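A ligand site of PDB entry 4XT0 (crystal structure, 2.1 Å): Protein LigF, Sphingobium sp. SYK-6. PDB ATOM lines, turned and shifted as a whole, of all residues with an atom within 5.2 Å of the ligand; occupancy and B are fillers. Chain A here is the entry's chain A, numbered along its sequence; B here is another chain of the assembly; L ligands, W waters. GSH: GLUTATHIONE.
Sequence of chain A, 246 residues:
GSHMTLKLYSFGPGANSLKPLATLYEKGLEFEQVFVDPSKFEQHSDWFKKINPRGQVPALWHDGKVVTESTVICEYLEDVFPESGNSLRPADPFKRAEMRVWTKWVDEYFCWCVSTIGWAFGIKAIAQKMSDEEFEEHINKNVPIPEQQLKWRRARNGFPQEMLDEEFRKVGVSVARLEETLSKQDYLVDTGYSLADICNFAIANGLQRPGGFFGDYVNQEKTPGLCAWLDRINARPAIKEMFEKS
OG of Ser 70 is in hydrogen-bond range of OD1 of Asn 16.
The side-chain hydroxyl of Ser 70 lies within hydrogen-bond range of the side-chain amino group of Lys 19.
OE1 of Glu 69 is in salt-bridge range of NZ of Lys 104 of chain B, 2.8 Å away.
The side-chain amide nitrogen (NE2) of Gln 148 lies close to the side-chain amide nitrogen (NE2) of Gln 56 (3.3 Å).
NZ of Lys 19 is in hydrogen-bond range of OD1 of Asn 16 (3.4 Å).
N of Phe 11 is in hydrogen-bond range of OG of Ser 17, 2.9 Å away.
An oxygen (O11) of the ligand sits at hydrogen-bond distance from the backbone NH (N) of Ser 70.
The side-chain hydroxyl of Ser 70 is in hydrogen-bond range of an oxygen (O12) of the ligand (2.7 Å).
The side-chain carboxylate (OE1) of Glu 69 is in salt-bridge range of a nitrogen (N1) of the ligand, 2.7 Å away.
O2 of the ligand sits at hydrogen-bond distance from N of Val 57 (3.2 Å).
The backbone carbonyl oxygen of Val 57 is in hydrogen-bond range of a nitrogen (N2) of the ligand, 2.7 Å away.
NE2 of Gln 56 is in hydrogen-bond range of O32 of the ligand (2.8 Å).
O31 of the ligand is in hydrogen-bond range of NE2 of Gln 43 (3.1 Å).
O31 of the ligand lies within hydrogen-bond range of NE1 of Trp 152 (3.1 Å).
NE2 of His 44 is in hydrogen-bond range of O31 of the ligand (3.1 Å).
NE2 of Gln 148 lies within hydrogen-bond range of O32 of the ligand.
The backbone NH (N) of Asn 16 sits close to a sulfur (SG2) of the ligand, 3.6 Å away.
SG2 of the ligand sits close to ND2 of Asn 16, 3.2 Å away.
Merely in contact with the ligand: Phe 11 (3.8 Å), Ala 15 (3.6 Å) and Pro 58 (3.7 Å).
Within 4 Å of the ligand: Phe 11, Ala 15, Asn 16, Gln 43, His 44, Gln 56, Val 57, Pro 58, Glu 69, Ser 70, Gln 148 and Trp 152.
Along chain A the residues within 4 Å of the ligand span positions 11 to 152.
The nearest printed residue that does not touch the ligand is Trp 119 (4.2 Å).
Water W5 lies within hydrogen-bond range of an oxygen (O32) of the ligand (2.6 Å) and a ring nitrogen (NE2) of His 44 (3.2 Å).
Water W2 lies within hydrogen-bond range of the backbone carbonyl oxygen (O) of Pro 58 (2.7 Å), an oxygen (O11) of the ligand (2.8 Å) and the backbone NH (N) of Glu 69 (2.9 Å).
Water W3 lies within hydrogen-bond range of NZ of Lys 104 of chain B (2.7 Å), OD1 of Asp 107 (2.7 Å), O12 of the ligand (2.9 Å), OG1 of Thr 71 (3.1 Å) and OG of Ser 70 (3.2 Å).
Water W8 bridges N3 of the ligand and NE1 of Trp 119.
Water W7 lies within hydrogen-bond range of the side-chain amide oxygen (OE1) of Gln 148 (2.9 Å), an oxygen (OE1) of the ligand (3.0 Å) and the side-chain amide nitrogen (NE2) of Gln 56 (3.4 Å).
Water W9 bridges the side-chain carboxylate of Glu 69 (2.6 Å) and a nitrogen (N1) of the ligand (3.3 Å).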
ATOM      1  N   PHE A  11     -15.071  26.297  16.986  1.00  0.00           N
ATOM      2  CA  PHE A  11     -15.309  27.023  15.734  1.00  0.00           C
ATOM      3  C   PHE A  11     -16.562  26.525  15.003  1.00  0.00           C
ATOM      4  O   PHE A  11     -16.806  26.936  13.868  1.00  0.00           O
ATOM      5  CB  PHE A  11     -14.105  26.899  14.772  1.00  0.00           C
ATOM      6  CG  PHE A  11     -12.880  27.684  15.193  1.00  0.00           C
ATOM      7  CD1 PHE A  11     -12.968  28.718  16.112  1.00  0.00           C
ATOM      8  CD2 PHE A  11     -11.643  27.375  14.652  1.00  0.00           C
ATOM      9  CE1 PHE A  11     -11.833  29.436  16.490  1.00  0.00           C
ATOM     10  CE2 PHE A  11     -10.509  28.083  15.020  1.00  0.00           C
ATOM     11  CZ  PHE A  11     -10.598  29.116  15.940  1.00  0.00           C
ATOM     12  N   ALA A  15     -13.322  20.445  11.174  1.00  0.00           N
ATOM     13  CA  ALA A  15     -12.004  20.155  11.725  1.00  0.00           C
ATOM     14  C   ALA A  15     -12.100  19.677  13.169  1.00  0.00           C
ATOM     15  O   ALA A  15     -12.993  18.904  13.515  1.00  0.00           O
ATOM     16  CB  ALA A  15     -11.090  21.413  11.620  1.00  0.00           C
ATOM     17  N   ASN A  16     -11.195  20.125  14.026  1.00  0.00           N
ATOM     18  CA  ASN A  16     -11.103  19.514  15.358  1.00  0.00           C
ATOM     19  C   ASN A  16     -12.330  19.811  16.214  1.00  0.00           C
ATOM     20  O   ASN A  16     -12.738  18.978  17.032  1.00  0.00           O
ATOM     21  CB  ASN A  16      -9.823  19.976  16.059  1.00  0.00           C
ATOM     22  CG  ASN A  16      -8.582  19.328  15.470  1.00  0.00           C
ATOM     23  OD1 ASN A  16      -8.490  18.103  15.413  1.00  0.00           O
ATOM     24  ND2 ASN A  16      -7.652  20.146  15.003  1.00  0.00           N
ATOM     25  N   SER A  17     -12.943  20.965  15.988  1.00  0.00           N
ATOM     26  CA  SER A  17     -14.168  21.352  16.705  1.00  0.00           C
ATOM     27  C   SER A  17     -15.339  20.378  16.473  1.00  0.00           C
ATOM     28  O   SER A  17     -16.159  20.171  17.360  1.00  0.00           O
ATOM     29  CB  SER A  17     -14.605  22.771  16.290  1.00  0.00           C
ATOM     30  OG  SER A  17     -13.705  23.757  16.783  1.00  0.00           O
ATOM     31  N   LYS A  19     -15.460  17.197  16.292  1.00  0.00           N
ATOM     32  CA  LYS A  19     -15.420  15.931  17.025  1.00  0.00           C
ATOM     33  C   LYS A  19     -16.271  15.990  18.307  1.00  0.00           C
ATOM     34  O   LYS A  19     -17.224  15.221  18.423  1.00  0.00           O
ATOM     35  CB  LYS A  19     -13.966  15.514  17.334  1.00  0.00           C
ATOM     36  CG  LYS A  19     -13.016  15.466  16.111  1.00  0.00           C
ATOM     37  CD  LYS A  19     -11.635  14.895  16.538  1.00  0.00           C
ATOM     38  CE  LYS A  19     -10.517  15.140  15.517  1.00  0.00           C
ATOM     39  NZ  LYS A  19      -9.175  14.807  16.108  1.00  0.00           N
ATOM     40  N   GLN A  43     -10.004  33.170  19.729  1.00  0.00           N
ATOM     41  CA  GLN A  43      -9.280  32.075  20.410  1.00  0.00           C
ATOM     42  C   GLN A  43      -8.031  32.640  21.092  1.00  0.00           C
ATOM     43  O   GLN A  43      -7.397  31.969  21.908  1.00  0.00           O
ATOM     44  CB  GLN A  43      -8.925  30.929  19.453  1.00  0.00           C
ATOM     45  CG  GLN A  43      -7.823  31.223  18.436  1.00  0.00           C
ATOM     46  CD  GLN A  43      -8.351  31.902  17.178  1.00  0.00           C
ATOM     47  OE1 GLN A  43      -9.385  32.565  17.209  1.00  0.00           O
ATOM     48  NE2 GLN A  43      -7.637  31.737  16.062  1.00  0.00           N
ATOM     49  N   HIS A  44      -7.677  33.888  20.755  1.00  0.00           N
ATOM     50  CA  HIS A  44      -6.513  34.538  21.334  1.00  0.00           C
ATOM     51  C   HIS A  44      -6.915  35.652  22.284  1.00  0.00           C
ATOM     52  O   HIS A  44      -6.070  36.426  22.745  1.00  0.00           O
ATOM     53  CB  HIS A  44      -5.610  35.098  20.228  1.00  0.00           C
ATOM     54  CG  HIS A  44      -5.130  34.068  19.274  1.00  0.00           C
ATOM     55  ND1 HIS A  44      -4.808  34.351  17.963  1.00  0.00           N
ATOM     56  CD2 HIS A  44      -4.915  32.740  19.425  1.00  0.00           C
ATOM     57  CE1 HIS A  44      -4.420  33.255  17.343  1.00  0.00           C
ATOM     58  NE2 HIS A  44      -4.480  32.250  18.210  1.00  0.00           N
ATOM     59  N   GLY A  55      -4.873  28.703  23.870  1.00  0.00           N
ATOM     60  CA  GLY A  55      -5.428  29.593  22.863  1.00  0.00           C
ATOM     61  C   GLY A  55      -5.912  28.886  21.607  1.00  0.00           C
ATOM     62  O   GLY A  55      -5.817  29.423  20.488  1.00  0.00           O
ATOM     63  N   GLN A  56      -6.436  27.682  21.790  1.00  0.00           N
ATOM     64  CA  GLN A  56      -6.999  26.914  20.681  1.00  0.00           C
ATOM     65  C   GLN A  56      -8.319  26.279  21.065  1.00  0.00           C
ATOM     66  O   GLN A  56      -8.645  26.117  22.238  1.00  0.00           O
ATOM     67  CB  GLN A  56      -6.006  25.849  20.197  1.00  0.00           C
ATOM     68  CG  GLN A  56      -4.888  26.422  19.330  1.00  0.00           C
ATOM     69  CD  GLN A  56      -4.067  25.347  18.636  1.00  0.00           C
ATOM     70  OE1 GLN A  56      -3.635  24.376  19.255  1.00  0.00           O
ATOM     71  NE2 GLN A  56      -3.855  25.530  17.332  1.00  0.00           N
ATOM     72  N   VAL A  57      -9.096  25.944  20.036  1.00  0.00           N
ATOM     73  CA  VAL A  57     -10.363  25.264  20.236  1.00  0.00           C
ATOM     74  C   VAL A  57     -10.197  23.831  19.724  1.00  0.00           C
ATOM     75  O   VAL A  57      -9.308  23.565  18.916  1.00  0.00           O
ATOM     76  CB  VAL A  57     -11.525  25.980  19.497  1.00  0.00           C
ATOM     77  CG1 VAL A  57     -11.733  27.398  20.035  1.00  0.00           C
ATOM     78  CG2 VAL A  57     -11.281  26.018  17.963  1.00  0.00           C
ATOM     79  N   PRO A  58     -11.044  22.884  20.182  1.00  0.00           N
ATOM     80  CA  PRO A  58     -12.148  23.045  21.143  1.00  0.00           C
ATOM     81  C   PRO A  58     -11.721  22.940  22.599  1.00  0.00           C
ATOM     82  O   PRO A  58     -10.647  22.424  22.936  1.00  0.00           O
ATOM     83  CB  PRO A  58     -13.082  21.888  20.778  1.00  0.00           C
ATOM     84  CG  PRO A  58     -12.139  20.820  20.352  1.00  0.00           C
ATOM     85  CD  PRO A  58     -11.106  21.568  19.527  1.00  0.00           C
ATOM     86  N   GLU A  69      -8.130  19.148  23.967  1.00  0.00           N
ATOM     87  CA  GLU A  69      -7.791  18.134  22.946  1.00  0.00           C
ATOM     88  C   GLU A  69      -9.059  17.443  22.425  1.00  0.00           C
ATOM     89  O   GLU A  69      -9.682  16.689  23.147  1.00  0.00           O
ATOM     90  CB  GLU A  69      -6.799  17.079  23.480  1.00  0.00           C
ATOM     91  CG  GLU A  69      -5.445  17.661  23.866  1.00  0.00           C
ATOM     92  CD  GLU A  69      -4.708  18.241  22.674  1.00  0.00           C
ATOM     93  OE1 GLU A  69      -4.598  17.541  21.634  1.00  0.00           O
ATOM     94  OE2 GLU A  69      -4.275  19.404  22.765  1.00  0.00           O
ATOM     95  N   SER A  70      -9.423  17.713  21.165  1.00  0.00           N
ATOM     96  CA  SER A  70     -10.675  17.200  20.596  1.00  0.00           C
ATOM     97  C   SER A  70     -10.916  15.704  20.868  1.00  0.00           C
ATOM     98  O   SER A  70     -11.991  15.333  21.352  1.00  0.00           O
ATOM     99  CB  SER A  70     -10.706  17.474  19.085  1.00  0.00           C
ATOM    100  OG  SER A  70      -9.571  16.917  18.424  1.00  0.00           O
ATOM    101  N   THR A  71      -9.926  14.859  20.601  1.00  0.00           N
ATOM    102  CA  THR A  71     -10.098  13.412  20.802  1.00  0.00           C
ATOM    103  C   THR A  71     -10.351  13.066  22.280  1.00  0.00           C
ATOM    104  O   THR A  71     -11.143  12.182  22.584  1.00  0.00           O
ATOM    105  CB  THR A  71      -8.862  12.641  20.294  1.00  0.00           C
ATOM    106  OG1 THR A  71      -8.684  12.897  18.899  1.00  0.00           O
ATOM    107  CG2 THR A  71      -9.025  11.099  20.532  1.00  0.00           C
ATOM    108  N   ASP A 107      -5.225  12.178  14.630  1.00  0.00           N
ATOM    109  CA  ASP A 107      -4.357  13.135  15.372  1.00  0.00           C
ATOM    110  C   ASP A 107      -2.911  13.169  14.906  1.00  0.00           C
ATOM    111  O   ASP A 107      -2.244  14.203  15.059  1.00  0.00           O
ATOM    112  CB  ASP A 107      -4.371  12.806  16.878  1.00  0.00           C
ATOM    113  CG  ASP A 107      -5.661  13.270  17.571  1.00  0.00           C
ATOM    114  OD1 ASP A 107      -6.225  14.315  17.188  1.00  0.00           O
ATOM    115  OD2 ASP A 107      -6.108  12.582  18.517  1.00  0.00           O
ATOM    116  N   TRP A 112      -3.331  16.565   9.958  1.00  0.00           N
ATOM    117  CA  TRP A 112      -2.276  17.532   9.690  1.00  0.00           C
ATOM    118  C   TRP A 112      -1.976  17.778   8.204  1.00  0.00           C
ATOM    119  O   TRP A 112      -1.662  18.918   7.813  1.00  0.00           O
ATOM    120  CB  TRP A 112      -0.995  17.132  10.441  1.00  0.00           C
ATOM    121  CG  TRP A 112      -1.214  17.051  11.921  1.00  0.00           C
ATOM    122  CD1 TRP A 112      -0.767  16.067  12.769  1.00  0.00           C
ATOM    123  CD2 TRP A 112      -1.961  17.970  12.752  1.00  0.00           C
ATOM    124  NE1 TRP A 112      -1.173  16.329  14.054  1.00  0.00           N
ATOM    125  CE2 TRP A 112      -1.907  17.481  14.069  1.00  0.00           C
ATOM    126  CE3 TRP A 112      -2.674  19.162  12.499  1.00  0.00           C
ATOM    127  CZ2 TRP A 112      -2.533  18.142  15.136  1.00  0.00           C
ATOM    128  CZ3 TRP A 112      -3.291  19.805  13.563  1.00  0.00           C
ATOM    129  CH2 TRP A 112      -3.212  19.298  14.860  1.00  0.00           C
ATOM    130  N   TRP A 119      -4.320  25.822   5.836  1.00  0.00           N
ATOM    131  CA  TRP A 119      -3.602  27.032   6.260  1.00  0.00           C
ATOM    132  C   TRP A 119      -3.016  27.790   5.060  1.00  0.00           C
ATOM    133  O   TRP A 119      -2.958  29.020   5.064  1.00  0.00           O
ATOM    134  CB  TRP A 119      -2.479  26.692   7.245  1.00  0.00           C
ATOM    135  CG  TRP A 119      -2.955  26.503   8.661  1.00  0.00           C
ATOM    136  CD1 TRP A 119      -3.422  25.339   9.229  1.00  0.00           C
ATOM    137  CD2 TRP A 119      -3.031  27.507   9.682  1.00  0.00           C
ATOM    138  NE1 TRP A 119      -3.768  25.567  10.535  1.00  0.00           N
ATOM    139  CE2 TRP A 119      -3.539  26.875  10.844  1.00  0.00           C
ATOM    140  CE3 TRP A 119      -2.704  28.855   9.738  1.00  0.00           C
ATOM    141  CZ2 TRP A 119      -3.734  27.577  12.038  1.00  0.00           C
ATOM    142  CZ3 TRP A 119      -2.901  29.547  10.922  1.00  0.00           C
ATOM    143  CH2 TRP A 119      -3.406  28.898  12.059  1.00  0.00           C
ATOM    144  N   GLN A 148       2.297  27.360  15.872  1.00  0.00           N
ATOM    145  CA  GLN A 148       1.146  28.079  15.337  1.00  0.00           C
ATOM    146  C   GLN A 148       1.524  29.500  14.894  1.00  0.00           C
ATOM    147  O   GLN A 148       0.901  30.060  13.995  1.00  0.00           O
ATOM    148  CB  GLN A 148       0.011  28.140  16.371  1.00  0.00           C
ATOM    149  CG  GLN A 148      -0.491  26.767  16.834  1.00  0.00           C
ATOM    150  CD  GLN A 148      -0.978  25.911  15.675  1.00  0.00           C
ATOM    151  OE1 GLN A 148      -0.568  24.758  15.528  1.00  0.00           O
ATOM    152  NE2 GLN A 148      -1.866  26.473  14.846  1.00  0.00           N
ATOM    153  N   TRP A 152       0.634  30.746  11.073  1.00  0.00           N
ATOM    154  CA  TRP A 152      -0.023  32.014  10.757  1.00  0.00           C
ATOM    155  C   TRP A 152       0.809  32.840   9.771  1.00  0.00           C
ATOM    156  O   TRP A 152       0.273  33.408   8.822  1.00  0.00           O
ATOM    157  CB  TRP A 152      -0.313  32.819  12.041  1.00  0.00           C
ATOM    158  CG  TRP A 152      -1.602  32.437  12.714  1.00  0.00           C
ATOM    159  CD1 TRP A 152      -1.746  31.790  13.911  1.00  0.00           C
ATOM    160  CD2 TRP A 152      -2.930  32.654  12.213  1.00  0.00           C
ATOM    161  NE1 TRP A 152      -3.085  31.590  14.192  1.00  0.00           N
ATOM    162  CE2 TRP A 152      -3.827  32.111  13.162  1.00  0.00           C
ATOM    163  CE3 TRP A 152      -3.444  33.248  11.051  1.00  0.00           C
ATOM    164  CZ2 TRP A 152      -5.214  32.156  12.985  1.00  0.00           C
ATOM    165  CZ3 TRP A 152      -4.824  33.294  10.881  1.00  0.00           C
ATOM    166  CH2 TRP A 152      -5.691  32.751  11.845  1.00  0.00           C
ATOM    167  N   LYS B 104      -1.046  11.384  24.435  1.00  0.00           N
ATOM    168  CA  LYS B 104      -1.147  11.724  23.027  1.00  0.00           C
ATOM    169  C   LYS B 104      -0.075  12.757  22.665  1.00  0.00           C
ATOM    170  O   LYS B 104       0.386  12.805  21.530  1.00  0.00           O
ATOM    171  CB  LYS B 104      -2.561  12.218  22.670  1.00  0.00           C
ATOM    172  CG  LYS B 104      -2.850  13.686  23.068  1.00  0.00           C
ATOM    173  CD  LYS B 104      -4.371  13.920  23.066  1.00  0.00           C
ATOM    174  CE  LYS B 104      -4.988  13.717  21.659  1.00  0.00           C
ATOM    175  NZ  LYS B 104      -4.572  14.841  20.727  1.00  0.00           N
ATOM    176  N   GLU B 108       2.352  12.636  19.523  1.00  0.00           N
ATOM    177  CA  GLU B 108       2.236  13.666  18.483  1.00  0.00           C
ATOM    178  C   GLU B 108       3.380  14.662  18.467  1.00  0.00           C
ATOM    179  O   GLU B 108       3.483  15.463  17.546  1.00  0.00           O
ATOM    180  CB  GLU B 108       0.916  14.429  18.664  1.00  0.00           C
ATOM    181  CG  GLU B 108      -0.304  13.507  18.546  1.00  0.00           C
ATOM    182  CD  GLU B 108      -1.584  14.108  19.110  1.00  0.00           C
ATOM    183  OE1 GLU B 108      -1.678  15.358  19.151  1.00  0.00           O
ATOM    184  OE2 GLU B 108      -2.500  13.324  19.505  1.00  0.00           O
HETATM  185  N1  GSH L   1      -4.535  18.944  19.284  1.00  0.00           N
HETATM  186  CA1 GSH L   1      -5.623  19.936  19.354  1.00  0.00           C
HETATM  187  C1  GSH L   1      -7.006  19.293  19.353  1.00  0.00           C
HETATM  188  O11 GSH L   1      -7.913  19.784  19.988  1.00  0.00           O
HETATM  189  O12 GSH L   1      -7.242  18.177  18.652  1.00  0.00           O
HETATM  190  CB1 GSH L   1      -5.488  20.878  18.138  1.00  0.00           C
HETATM  191  CG1 GSH L   1      -6.506  22.007  18.297  1.00  0.00           C
HETATM  192  CD1 GSH L   1      -6.495  22.885  17.054  1.00  0.00           C
HETATM  193  OE1 GSH L   1      -5.627  22.740  16.216  1.00  0.00           O
HETATM  194  N2  GSH L   1      -7.457  23.818  16.905  1.00  0.00           N
HETATM  195  CA2 GSH L   1      -7.467  24.695  15.720  1.00  0.00           C
HETATM  196  C2  GSH L   1      -7.301  26.133  16.169  1.00  0.00           C
HETATM  197  O2  GSH L   1      -7.625  26.449  17.292  1.00  0.00           O
HETATM  198  CB2 GSH L   1      -8.834  24.578  15.019  1.00  0.00           C
HETATM  199  SG2 GSH L   1      -9.050  22.964  14.205  1.00  0.00           S
HETATM  200  N3  GSH L   1      -6.806  27.073  15.310  1.00  0.00           N
HETATM  201  CA3 GSH L   1      -6.694  28.470  15.772  1.00  0.00           C
HETATM  202  C3  GSH L   1      -5.270  28.928  16.013  1.00  0.00           C
HETATM  203  O31 GSH L   1      -5.047  30.114  16.056  1.00  0.00           O
HETATM  204  O32 GSH L   1      -4.263  28.049  16.166  1.00  0.00           O
HETATM  205  O   HOH W   1     -12.021  23.407  14.586  1.00  0.00           O
HETATM  206  O   HOH W   2      -8.184  21.491  22.203  1.00  0.00           O
HETATM  207  O   HOH W   3      -6.966  15.449  19.570  1.00  0.00           O
HETATM  208  O   HOH W   4      -4.433  16.377  17.630  1.00  0.00           O
HETATM  209  O   HOH W   5      -3.008  29.429  18.020  1.00  0.00           O
HETATM  210  O   HOH W   6      -2.000  19.782  18.404  1.00  0.00           O
HETATM  211  O   HOH W   7      -2.649  22.760  15.809  1.00  0.00           O
HETATM  212  O   HOH W   8      -6.438  25.654  12.796  1.00  0.00           O
HETATM  213  O   HOH W   9      -2.518  20.627  21.261  1.00  0.00           O
